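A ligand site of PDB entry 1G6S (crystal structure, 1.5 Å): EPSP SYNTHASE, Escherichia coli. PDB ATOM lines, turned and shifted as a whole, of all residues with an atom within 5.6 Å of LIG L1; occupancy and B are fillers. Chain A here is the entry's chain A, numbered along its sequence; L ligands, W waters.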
ATOM      1  N   LYS A  22       1.060 -12.007  20.350  1.00  0.00           N
ATOM      2  CA  LYS A  22      -0.384 -12.273  20.385  1.00  0.00           C
ATOM      3  C   LYS A  22      -0.690 -13.571  21.169  1.00  0.00           C
ATOM      4  O   LYS A  22      -1.647 -13.604  21.982  1.00  0.00           O
ATOM      5  CB  LYS A  22      -0.910 -12.377  18.939  1.00  0.00           C
ATOM      6  CG  LYS A  22      -2.405 -12.802  18.825  1.00  0.00           C
ATOM      7  CD  LYS A  22      -2.534 -14.204  18.173  1.00  0.00           C
ATOM      8  CE  LYS A  22      -2.352 -14.105  16.640  1.00  0.00           C
ATOM      9  NZ  LYS A  22      -2.232 -15.472  16.047  1.00  0.00           N
ATOM     10  N   SER A  23       0.070 -14.622  20.888  1.00  0.00           N
ATOM     11  CA  SER A  23      -0.145 -15.929  21.544  1.00  0.00           C
ATOM     12  C   SER A  23      -0.002 -15.824  23.061  1.00  0.00           C
ATOM     13  O   SER A  23      -0.827 -16.384  23.812  1.00  0.00           O
ATOM     14  CB  SER A  23       0.857 -16.934  20.995  1.00  0.00           C
ATOM     15  OG  SER A  23       0.564 -17.233  19.636  1.00  0.00           O
ATOM     16  N   ARG A  27      -3.275 -15.745  26.073  1.00  0.00           N
ATOM     17  CA  ARG A  27      -3.270 -16.754  27.140  1.00  0.00           C
ATOM     18  C   ARG A  27      -3.141 -16.050  28.495  1.00  0.00           C
ATOM     19  O   ARG A  27      -3.849 -16.391  29.467  1.00  0.00           O
ATOM     20  CB  ARG A  27      -2.067 -17.674  27.015  1.00  0.00           C
ATOM     21  CG  ARG A  27      -2.220 -18.731  25.924  1.00  0.00           C
ATOM     22  CD  ARG A  27      -0.845 -19.299  25.613  1.00  0.00           C
ATOM     23  NE  ARG A  27      -0.839 -20.446  24.691  1.00  0.00           N
ATOM     24  CZ  ARG A  27      -0.969 -20.367  23.369  1.00  0.00           C
ATOM     25  NH1 ARG A  27      -0.909 -21.481  22.620  1.00  0.00           N
ATOM     26  NH2 ARG A  27      -1.160 -19.178  22.773  1.00  0.00           N
ATOM     27  N   THR A  97      -7.198 -17.433  19.040  1.00  0.00           N
ATOM     28  CA  THR A  97      -6.661 -17.492  20.415  1.00  0.00           C
ATOM     29  C   THR A  97      -7.619 -16.961  21.432  1.00  0.00           C
ATOM     30  O   THR A  97      -7.337 -17.055  22.643  1.00  0.00           O
ATOM     31  CB  THR A  97      -5.280 -16.824  20.551  1.00  0.00           C
ATOM     32  OG1 THR A  97      -5.398 -15.437  20.210  1.00  0.00           O
ATOM     33  CG2 THR A  97      -4.237 -17.526  19.666  1.00  0.00           C
ATOM     34  N   ARG A 100     -11.007 -20.342  20.538  1.00  0.00           N
ATOM     35  CA  ARG A 100     -10.803 -21.703  21.004  1.00  0.00           C
ATOM     36  C   ARG A 100     -10.652 -21.766  22.537  1.00  0.00           C
ATOM     37  O   ARG A 100     -11.370 -22.520  23.201  1.00  0.00           O
ATOM     38  CB  ARG A 100      -9.599 -22.333  20.268  1.00  0.00           C
ATOM     39  CG  ARG A 100      -9.955 -22.916  18.877  1.00  0.00           C
ATOM     40  CD  ARG A 100     -10.290 -21.804  17.836  1.00  0.00           C
ATOM     41  NE  ARG A 100     -10.508 -22.354  16.502  1.00  0.00           N
ATOM     42  CZ  ARG A 100      -9.549 -22.487  15.564  1.00  0.00           C
ATOM     43  NH1 ARG A 100      -9.840 -22.984  14.368  1.00  0.00           N
ATOM     44  NH2 ARG A 100      -8.303 -22.113  15.819  1.00  0.00           N
ATOM     45  N   VAL A 168      -5.491 -30.856  13.104  1.00  0.00           N
ATOM     46  CA  VAL A 168      -5.874 -29.627  12.378  1.00  0.00           C
ATOM     47  C   VAL A 168      -5.441 -28.379  13.134  1.00  0.00           C
ATOM     48  O   VAL A 168      -4.976 -27.402  12.515  1.00  0.00           O
ATOM     49  CB  VAL A 168      -7.397 -29.631  12.120  1.00  0.00           C
ATOM     50  CG1 VAL A 168      -7.873 -28.279  11.550  1.00  0.00           C
ATOM     51  CG2 VAL A 168      -7.730 -30.739  11.146  1.00  0.00           C
ATOM     52  N   SER A 169      -5.600 -28.357  14.450  1.00  0.00           N
ATOM     53  CA  SER A 169      -5.114 -27.212  15.243  1.00  0.00           C
ATOM     54  C   SER A 169      -4.610 -27.674  16.581  1.00  0.00           C
ATOM     55  O   SER A 169      -5.255 -28.498  17.234  1.00  0.00           O
ATOM     56  CB  SER A 169      -6.260 -26.189  15.501  1.00  0.00           C
ATOM     57  OG  SER A 169      -5.762 -25.044  16.216  1.00  0.00           O
ATOM     58  N   SER A 170      -3.513 -27.084  17.021  1.00  0.00           N
ATOM     59  CA  SER A 170      -3.018 -27.330  18.361  1.00  0.00           C
ATOM     60  C   SER A 170      -3.886 -26.535  19.368  1.00  0.00           C
ATOM     61  O   SER A 170      -3.838 -26.812  20.573  1.00  0.00           O
ATOM     62  CB  SER A 170      -1.559 -26.833  18.526  1.00  0.00           C
ATOM     63  OG  SER A 170      -1.445 -25.401  18.451  1.00  0.00           O
ATOM     64  N   GLN A 171      -4.678 -25.575  18.897  1.00  0.00           N
ATOM     65  CA  GLN A 171      -5.456 -24.743  19.793  1.00  0.00           C
ATOM     66  C   GLN A 171      -6.537 -25.495  20.541  1.00  0.00           C
ATOM     67  O   GLN A 171      -6.926 -25.071  21.635  1.00  0.00           O
ATOM     68  CB  GLN A 171      -6.072 -23.580  19.038  1.00  0.00           C
ATOM     69  CG  GLN A 171      -5.021 -22.554  18.592  1.00  0.00           C
ATOM     70  CD  GLN A 171      -5.657 -21.343  17.959  1.00  0.00           C
ATOM     71  OE1 GLN A 171      -6.875 -21.127  18.040  1.00  0.00           O
ATOM     72  NE2 GLN A 171      -4.821 -20.488  17.349  1.00  0.00           N
ATOM     73  N   THR A 174      -4.643 -26.865  23.431  1.00  0.00           N
ATOM     74  CA  THR A 174      -4.352 -25.738  24.311  1.00  0.00           C
ATOM     75  C   THR A 174      -5.566 -25.342  25.159  1.00  0.00           C
ATOM     76  O   THR A 174      -5.452 -25.131  26.373  1.00  0.00           O
ATOM     77  CB  THR A 174      -3.880 -24.515  23.469  1.00  0.00           C
ATOM     78  OG1 THR A 174      -2.473 -24.666  23.273  1.00  0.00           O
ATOM     79  CG2 THR A 174      -4.191 -23.163  24.159  1.00  0.00           C
ATOM     80  N   VAL A 196      -0.213 -31.192  15.264  1.00  0.00           N
ATOM     81  CA  VAL A 196       0.437 -30.125  14.498  1.00  0.00           C
ATOM     82  C   VAL A 196       0.724 -28.929  15.401  1.00  0.00           C
ATOM     83  O   VAL A 196       0.205 -28.827  16.515  1.00  0.00           O
ATOM     84  CB  VAL A 196      -0.417 -29.633  13.311  1.00  0.00           C
ATOM     85  CG1 VAL A 196      -0.615 -30.791  12.296  1.00  0.00           C
ATOM     86  CG2 VAL A 196      -1.777 -29.061  13.780  1.00  0.00           C
ATOM     87  N   SER A 197       1.588 -28.050  14.922  1.00  0.00           N
ATOM     88  CA  SER A 197       1.897 -26.825  15.646  1.00  0.00           C
ATOM     89  C   SER A 197       2.289 -27.106  17.079  1.00  0.00           C
ATOM     90  O   SER A 197       1.978 -26.335  17.991  1.00  0.00           O
ATOM     91  CB  SER A 197       0.674 -25.912  15.604  1.00  0.00           C
ATOM     92  OG  SER A 197       0.595 -25.376  14.274  1.00  0.00           O
ATOM     93  N   TYR A 200       3.336 -24.555  20.049  1.00  0.00           N
ATOM     94  CA  TYR A 200       2.348 -23.756  20.757  1.00  0.00           C
ATOM     95  C   TYR A 200       1.839 -24.431  22.024  1.00  0.00           C
ATOM     96  O   TYR A 200       1.382 -23.723  22.967  1.00  0.00           O
ATOM     97  CB  TYR A 200       1.172 -23.350  19.849  1.00  0.00           C
ATOM     98  CG  TYR A 200       1.633 -22.347  18.800  1.00  0.00           C
ATOM     99  CD1 TYR A 200       2.040 -22.774  17.541  1.00  0.00           C
ATOM    100  CD2 TYR A 200       1.638 -20.959  19.066  1.00  0.00           C
ATOM    101  CE1 TYR A 200       2.446 -21.844  16.564  1.00  0.00           C
ATOM    102  CE2 TYR A 200       2.035 -20.049  18.066  1.00  0.00           C
ATOM    103  CZ  TYR A 200       2.445 -20.489  16.846  1.00  0.00           C
ATOM    104  OH  TYR A 200       2.869 -19.610  15.856  1.00  0.00           O
ATOM    105  N   ILE A 203       4.018 -23.242  24.701  1.00  0.00           N
ATOM    106  CA  ILE A 203       3.706 -21.910  25.171  1.00  0.00           C
ATOM    107  C   ILE A 203       2.565 -22.016  26.218  1.00  0.00           C
ATOM    108  O   ILE A 203       2.614 -21.384  27.248  1.00  0.00           O
ATOM    109  CB  ILE A 203       3.250 -21.038  23.990  1.00  0.00           C
ATOM    110  CG1 ILE A 203       4.408 -20.860  23.001  1.00  0.00           C
ATOM    111  CG2 ILE A 203       2.784 -19.684  24.497  1.00  0.00           C
ATOM    112  CD1 ILE A 203       4.006 -19.954  21.766  1.00  0.00           C
ATOM    113  N   THR A 204       1.542 -22.825  25.912  1.00  0.00           N
ATOM    114  CA  THR A 204       0.436 -23.003  26.850  1.00  0.00           C
ATOM    115  C   THR A 204       0.904 -23.540  28.213  1.00  0.00           C
ATOM    116  O   THR A 204       0.512 -22.987  29.246  1.00  0.00           O
ATOM    117  CB  THR A 204      -0.585 -23.964  26.255  1.00  0.00           C
ATOM    118  OG1 THR A 204      -1.065 -23.337  25.042  1.00  0.00           O
ATOM    119  CG2 THR A 204      -1.767 -24.212  27.214  1.00  0.00           C
ATOM    120  N   PRO A 312       4.325 -22.624  11.318  1.00  0.00           N
ATOM    121  CA  PRO A 312       3.397 -22.327  10.236  1.00  0.00           C
ATOM    122  C   PRO A 312       3.159 -20.881   9.886  1.00  0.00           C
ATOM    123  O   PRO A 312       2.933 -20.573   8.703  1.00  0.00           O
ATOM    124  CB  PRO A 312       2.114 -23.070  10.655  1.00  0.00           C
ATOM    125  CG  PRO A 312       2.153 -22.996  12.168  1.00  0.00           C
ATOM    126  CD  PRO A 312       3.641 -23.297  12.448  1.00  0.00           C
ATOM    127  N   ASP A 313       3.182 -20.022  10.899  1.00  0.00           N
ATOM    128  CA  ASP A 313       2.889 -18.587  10.667  1.00  0.00           C
ATOM    129  C   ASP A 313       4.102 -17.874  10.069  1.00  0.00           C
ATOM    130  O   ASP A 313       4.000 -17.253   9.006  1.00  0.00           O
ATOM    131  CB  ASP A 313       2.463 -17.908  11.967  1.00  0.00           C
ATOM    132  CG  ASP A 313       1.133 -18.424  12.523  1.00  0.00           C
ATOM    133  OD1 ASP A 313       0.786 -17.972  13.620  1.00  0.00           O
ATOM    134  OD2 ASP A 313       0.469 -19.260  11.892  1.00  0.00           O
ATOM    135  N   ASN A 336      -2.671 -26.771   7.459  1.00  0.00           N
ATOM    136  CA  ASN A 336      -3.589 -25.878   8.164  1.00  0.00           C
ATOM    137  C   ASN A 336      -3.512 -24.418   7.797  1.00  0.00           C
ATOM    138  O   ASN A 336      -4.303 -23.603   8.287  1.00  0.00           O
ATOM    139  CB  ASN A 336      -3.642 -26.181   9.675  1.00  0.00           C
ATOM    140  CG  ASN A 336      -2.521 -25.602  10.467  1.00  0.00           C
ATOM    141  OD1 ASN A 336      -1.659 -24.819   9.944  1.00  0.00           O
ATOM    142  ND2 ASN A 336      -2.479 -25.963  11.758  1.00  0.00           N
ATOM    143  N   LYS A 340      -6.986 -21.068   8.294  1.00  0.00           N
ATOM    144  CA  LYS A 340      -6.662 -19.915   9.123  1.00  0.00           C
ATOM    145  C   LYS A 340      -7.351 -18.618   8.653  1.00  0.00           C
ATOM    146  O   LYS A 340      -8.505 -18.702   8.231  1.00  0.00           O
ATOM    147  CB  LYS A 340      -5.145 -19.824   9.277  1.00  0.00           C
ATOM    148  CG  LYS A 340      -4.734 -20.953  10.296  1.00  0.00           C
ATOM    149  CD  LYS A 340      -3.243 -21.100  10.403  1.00  0.00           C
ATOM    150  CE  LYS A 340      -2.959 -22.052  11.587  1.00  0.00           C
ATOM    151  NZ  LYS A 340      -1.509 -22.441  11.658  1.00  0.00           N
ATOM    152  N   GLU A 341      -6.695 -17.449   8.697  1.00  0.00           N
ATOM    153  CA  GLU A 341      -7.389 -16.199   8.333  1.00  0.00           C
ATOM    154  C   GLU A 341      -8.008 -16.219   6.950  1.00  0.00           C
ATOM    155  O   GLU A 341      -9.026 -15.556   6.719  1.00  0.00           O
ATOM    156  CB  GLU A 341      -6.475 -14.980   8.495  1.00  0.00           C
ATOM    157  CG  GLU A 341      -6.237 -14.612   9.988  1.00  0.00           C
ATOM    158  CD  GLU A 341      -5.176 -15.454  10.738  1.00  0.00           C
ATOM    159  OE1 GLU A 341      -4.857 -16.607  10.336  1.00  0.00           O
ATOM    160  OE2 GLU A 341      -4.703 -14.945  11.784  1.00  0.00           O
ATOM    161  N   ARG A 344      -4.585 -19.942   3.106  1.00  0.00           N
ATOM    162  CA  ARG A 344      -3.291 -19.347   2.754  1.00  0.00           C
ATOM    163  C   ARG A 344      -2.532 -20.062   1.652  1.00  0.00           C
ATOM    164  O   ARG A 344      -1.693 -19.431   1.009  1.00  0.00           O
ATOM    165  CB  ARG A 344      -2.428 -19.204   4.040  1.00  0.00           C
ATOM    166  CG  ARG A 344      -3.014 -18.138   4.956  1.00  0.00           C
ATOM    167  CD  ARG A 344      -2.465 -18.303   6.379  1.00  0.00           C
ATOM    168  NE  ARG A 344      -2.570 -17.021   7.072  1.00  0.00           N
ATOM    169  CZ  ARG A 344      -2.084 -16.792   8.284  1.00  0.00           C
ATOM    170  NH1 ARG A 344      -2.176 -15.578   8.817  1.00  0.00           N
ATOM    171  NH2 ARG A 344      -1.570 -17.790   9.027  1.00  0.00           N
ATOM    172  N   ARG A 386      -1.117 -11.369   7.597  1.00  0.00           N
ATOM    173  CA  ARG A 386       0.169 -11.854   7.108  1.00  0.00           C
ATOM    174  C   ARG A 386       0.299 -11.802   5.609  1.00  0.00           C
ATOM    175  O   ARG A 386       1.429 -11.730   5.099  1.00  0.00           O
ATOM    176  CB  ARG A 386       0.490 -13.257   7.624  1.00  0.00           C
ATOM    177  CG  ARG A 386       0.624 -13.270   9.170  1.00  0.00           C
ATOM    178  CD  ARG A 386       1.481 -14.495   9.666  1.00  0.00           C
ATOM    179  NE  ARG A 386       1.227 -14.616  11.114  1.00  0.00           N
ATOM    180  CZ  ARG A 386       1.629 -13.743  12.038  1.00  0.00           C
ATOM    181  NH1 ARG A 386       1.185 -13.922  13.298  1.00  0.00           N
ATOM    182  NH2 ARG A 386       2.546 -12.800  11.782  1.00  0.00           N
HETATM  183  C1  LIG L   1      -1.464 -20.246  17.977  1.00  0.00           C
HETATM  184  C2  LIG L   1      -1.376 -21.498  17.365  1.00  0.00           C
HETATM  185  C3  LIG L   1      -1.308 -21.637  15.857  1.00  0.00           C
HETATM  186  C4  LIG L   1      -0.970 -20.312  15.154  1.00  0.00           C
HETATM  187  C5  LIG L   1      -1.809 -19.171  15.729  1.00  0.00           C
HETATM  188  C6  LIG L   1      -1.432 -19.022  17.212  1.00  0.00           C
HETATM  189  C7  LIG L   1      -1.529 -20.196  19.471  1.00  0.00           C
HETATM  190  O1  LIG L   1      -2.563 -22.248  15.354  1.00  0.00           O
HETATM  191  O2  LIG L   1      -1.176 -20.477  13.742  1.00  0.00           O
HETATM  192  O3  LIG L   1      -1.522 -17.951  15.034  1.00  0.00           O
HETATM  193  O4  LIG L   1      -1.911 -21.229  20.080  1.00  0.00           O
HETATM  194  O5  LIG L   1      -1.183 -19.145  20.005  1.00  0.00           O
HETATM  195  P1  LIG L   1      -2.668 -23.859  14.930  1.00  0.00           P
HETATM  196  O6  LIG L   1      -2.372 -24.659  16.142  1.00  0.00           O
HETATM  197  O7  LIG L   1      -1.635 -23.995  13.821  1.00  0.00           O
HETATM  198  O8  LIG L   1      -4.091 -23.994  14.468  1.00  0.00           O
HETATM  199  P1  LG2 L   2      -5.612 -17.608  14.946  1.00  0.00           P
HETATM  200  O1  LG2 L   2      -4.687 -17.008  15.918  1.00  0.00           O
HETATM  201  O2  LG2 L   2      -6.147 -18.909  15.335  1.00  0.00           O
HETATM  202  O3  LG2 L   2      -6.741 -16.648  14.557  1.00  0.00           O
HETATM  203  O4  LG2 L   2      -1.502 -15.464  13.224  1.00  0.00           O
HETATM  204  O5  LG2 L   2      -0.746 -16.323  11.316  1.00  0.00           O
HETATM  205  C1  LG2 L   2      -4.722 -18.020  13.495  1.00  0.00           C
HETATM  206  C2  LG2 L   2      -2.642 -17.331  12.204  1.00  0.00           C
HETATM  207  C3  LG2 L   2      -1.542 -16.281  12.240  1.00  0.00           C
HETATM  208  N1  LG2 L   2      -3.604 -17.098  13.333  1.00  0.00           N
HETATM  209  O   HOH W   1      -5.749 -21.682  14.356  1.00  0.00           O
HETATM  210  O   HOH W   2      -2.208 -23.928  20.669  1.00  0.00           O
HETATM  211  O   HOH W   3      -5.628 -24.506  12.377  1.00  0.00           O
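Thr 97 touches LIG L1 (CG2 to O5, 3.5 Å).
Tyr 200 touches LIG L1 (CD2 to C7, 3.3 Å).
Hydrophobic or aromatic side chains that line LIG L1: Tyr 200.
12 residues have an atom within 4 Å of LIG L1: Lys 22, Ser 23, Arg 27, Thr 97, Ser 169, Ser 170, Gln 171, Ser 197, Tyr 200, Asp 313, Asn 336 and Lys 340.
Water W3 lies within hydrogen-bond range of an oxygen (O8) of LIG L1 (2.6 Å) and the backbone carbonyl oxygen of Val 168 (3.0 Å).
Water W2 lies within hydrogen-bond range of the side-chain hydroxyl of Thr 174 (2.7 Å), the side-chain hydroxyl of Ser 170 (2.8 Å), an oxygen (O4) of LIG L1 (2.8 Å), the guanidinium group of Arg 27 (3.4 Å) and the backbone NH of Gln 171 (3.5 Å).
Water W1 lies within hydrogen-bond range of O8 of LIG L1 (2.8 Å), O2 of LG2 L2 (3.0 Å), NH2 of Arg 100 (3.0 Å) and NE2 of Gln 171 (3.4 Å).
The side-chain amino group (NZ) of Lys 340 is in salt-bridge range of the side-chain carboxylate (OD2) of Asp 313 (3.8 Å).
The side-chain amino group (NZ) of Lys 340 sits at hydrogen-bond distance from the side-chain amide oxygen (OD1) of Asn 336.
NH1 of Arg 27 sits at hydrogen-bond distance from O of Tyr 200 (3.2 Å).
The backbone carbonyl oxygen (O) of Tyr 200 sits at hydrogen-bond distance from the side-chain hydroxyl (OG1) of Thr 204.
ND2 of Asn 336 lies within hydrogen-bond range of O of Val 168 (3.0 Å).
The side-chain carboxylate (OD2) of Asp 313 is in salt-bridge range of the guanidinium group (NH2) of Arg 344 (3.8 Å).
OD1 of Asp 313 sits at hydrogen-bond distance from OH of Tyr 200 (3.5 Å).
NH2 of Arg 100 lies within hydrogen-bond range of OE1 of Gln 171 (2.8 Å).
An oxygen (O3) of LIG L1 lies within hydrogen-bond range of a nitrogen (N1) of LG2 L2 (2.8 Å).
The side-chain carboxylate of Asp 313 lies within hydrogen-bond range of an oxygen (O3) of LIG L1 (2.7 Å).
An oxygen (O2) of LG2 L2 sits at hydrogen-bond distance from the side-chain amide nitrogen (NE2) of Gln 171, at 2.9 Å.
NH2 of Arg 100 is in salt-bridge range of O2 of LG2 L2, 3.9 Å away.
The side-chain hydroxyl (OG) of Ser 23 sits at hydrogen-bond distance from an oxygen (O5) of LIG L1, at 2.6 Å.
A nitrogen (N1) of LG2 L2 is in salt-bridge range of the side-chain carboxylate of Glu 341 (2.9 Å).
An oxygen (O7) of LIG L1 is in hydrogen-bond range of the side-chain amide nitrogen (ND2) of Asn 336, at 3.0 Å.
The side-chain hydroxyl (OG) of Ser 197 is in hydrogen-bond range of an oxygen (O7) of LIG L1, at 2.7 Å.
The side-chain hydroxyl (OG) of Ser 170 is in hydrogen-bond range of an oxygen (O6) of LIG L1 (2.6 Å).
NZ of Lys 22 lies within salt-bridge range of O1 of LG2 L2 (2.9 Å).
An oxygen (O3) of LIG L1 sits at hydrogen-bond distance from the side-chain amino group of Lys 22, at 2.8 Å.
The guanidinium group (NH2) of Arg 344 lies within salt-bridge range of an oxygen (O5) of LG2 L2, 2.8 Å away.
The side-chain amino group (NZ) of Lys 340 lies within salt-bridge range of an oxygen (O7) of LIG L1, at 2.7 Å.
O1 of LIG L1 lies close to NE2 of Gln 171.
The backbone NH of Ser 170 is in hydrogen-bond range of an oxygen (O6) of LIG L1 (2.8 Å).
An oxygen (O8) of LIG L1 is in hydrogen-bond range of the side-chain hydroxyl (OG) of Ser 169 (2.6 Å).
NE of Arg 386 is in salt-bridge range of O5 of LG2 L2.
An oxygen (O4) of LIG L1 lies within salt-bridge range of the guanidinium group (NH1) of Arg 27, 2.7 Å away.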
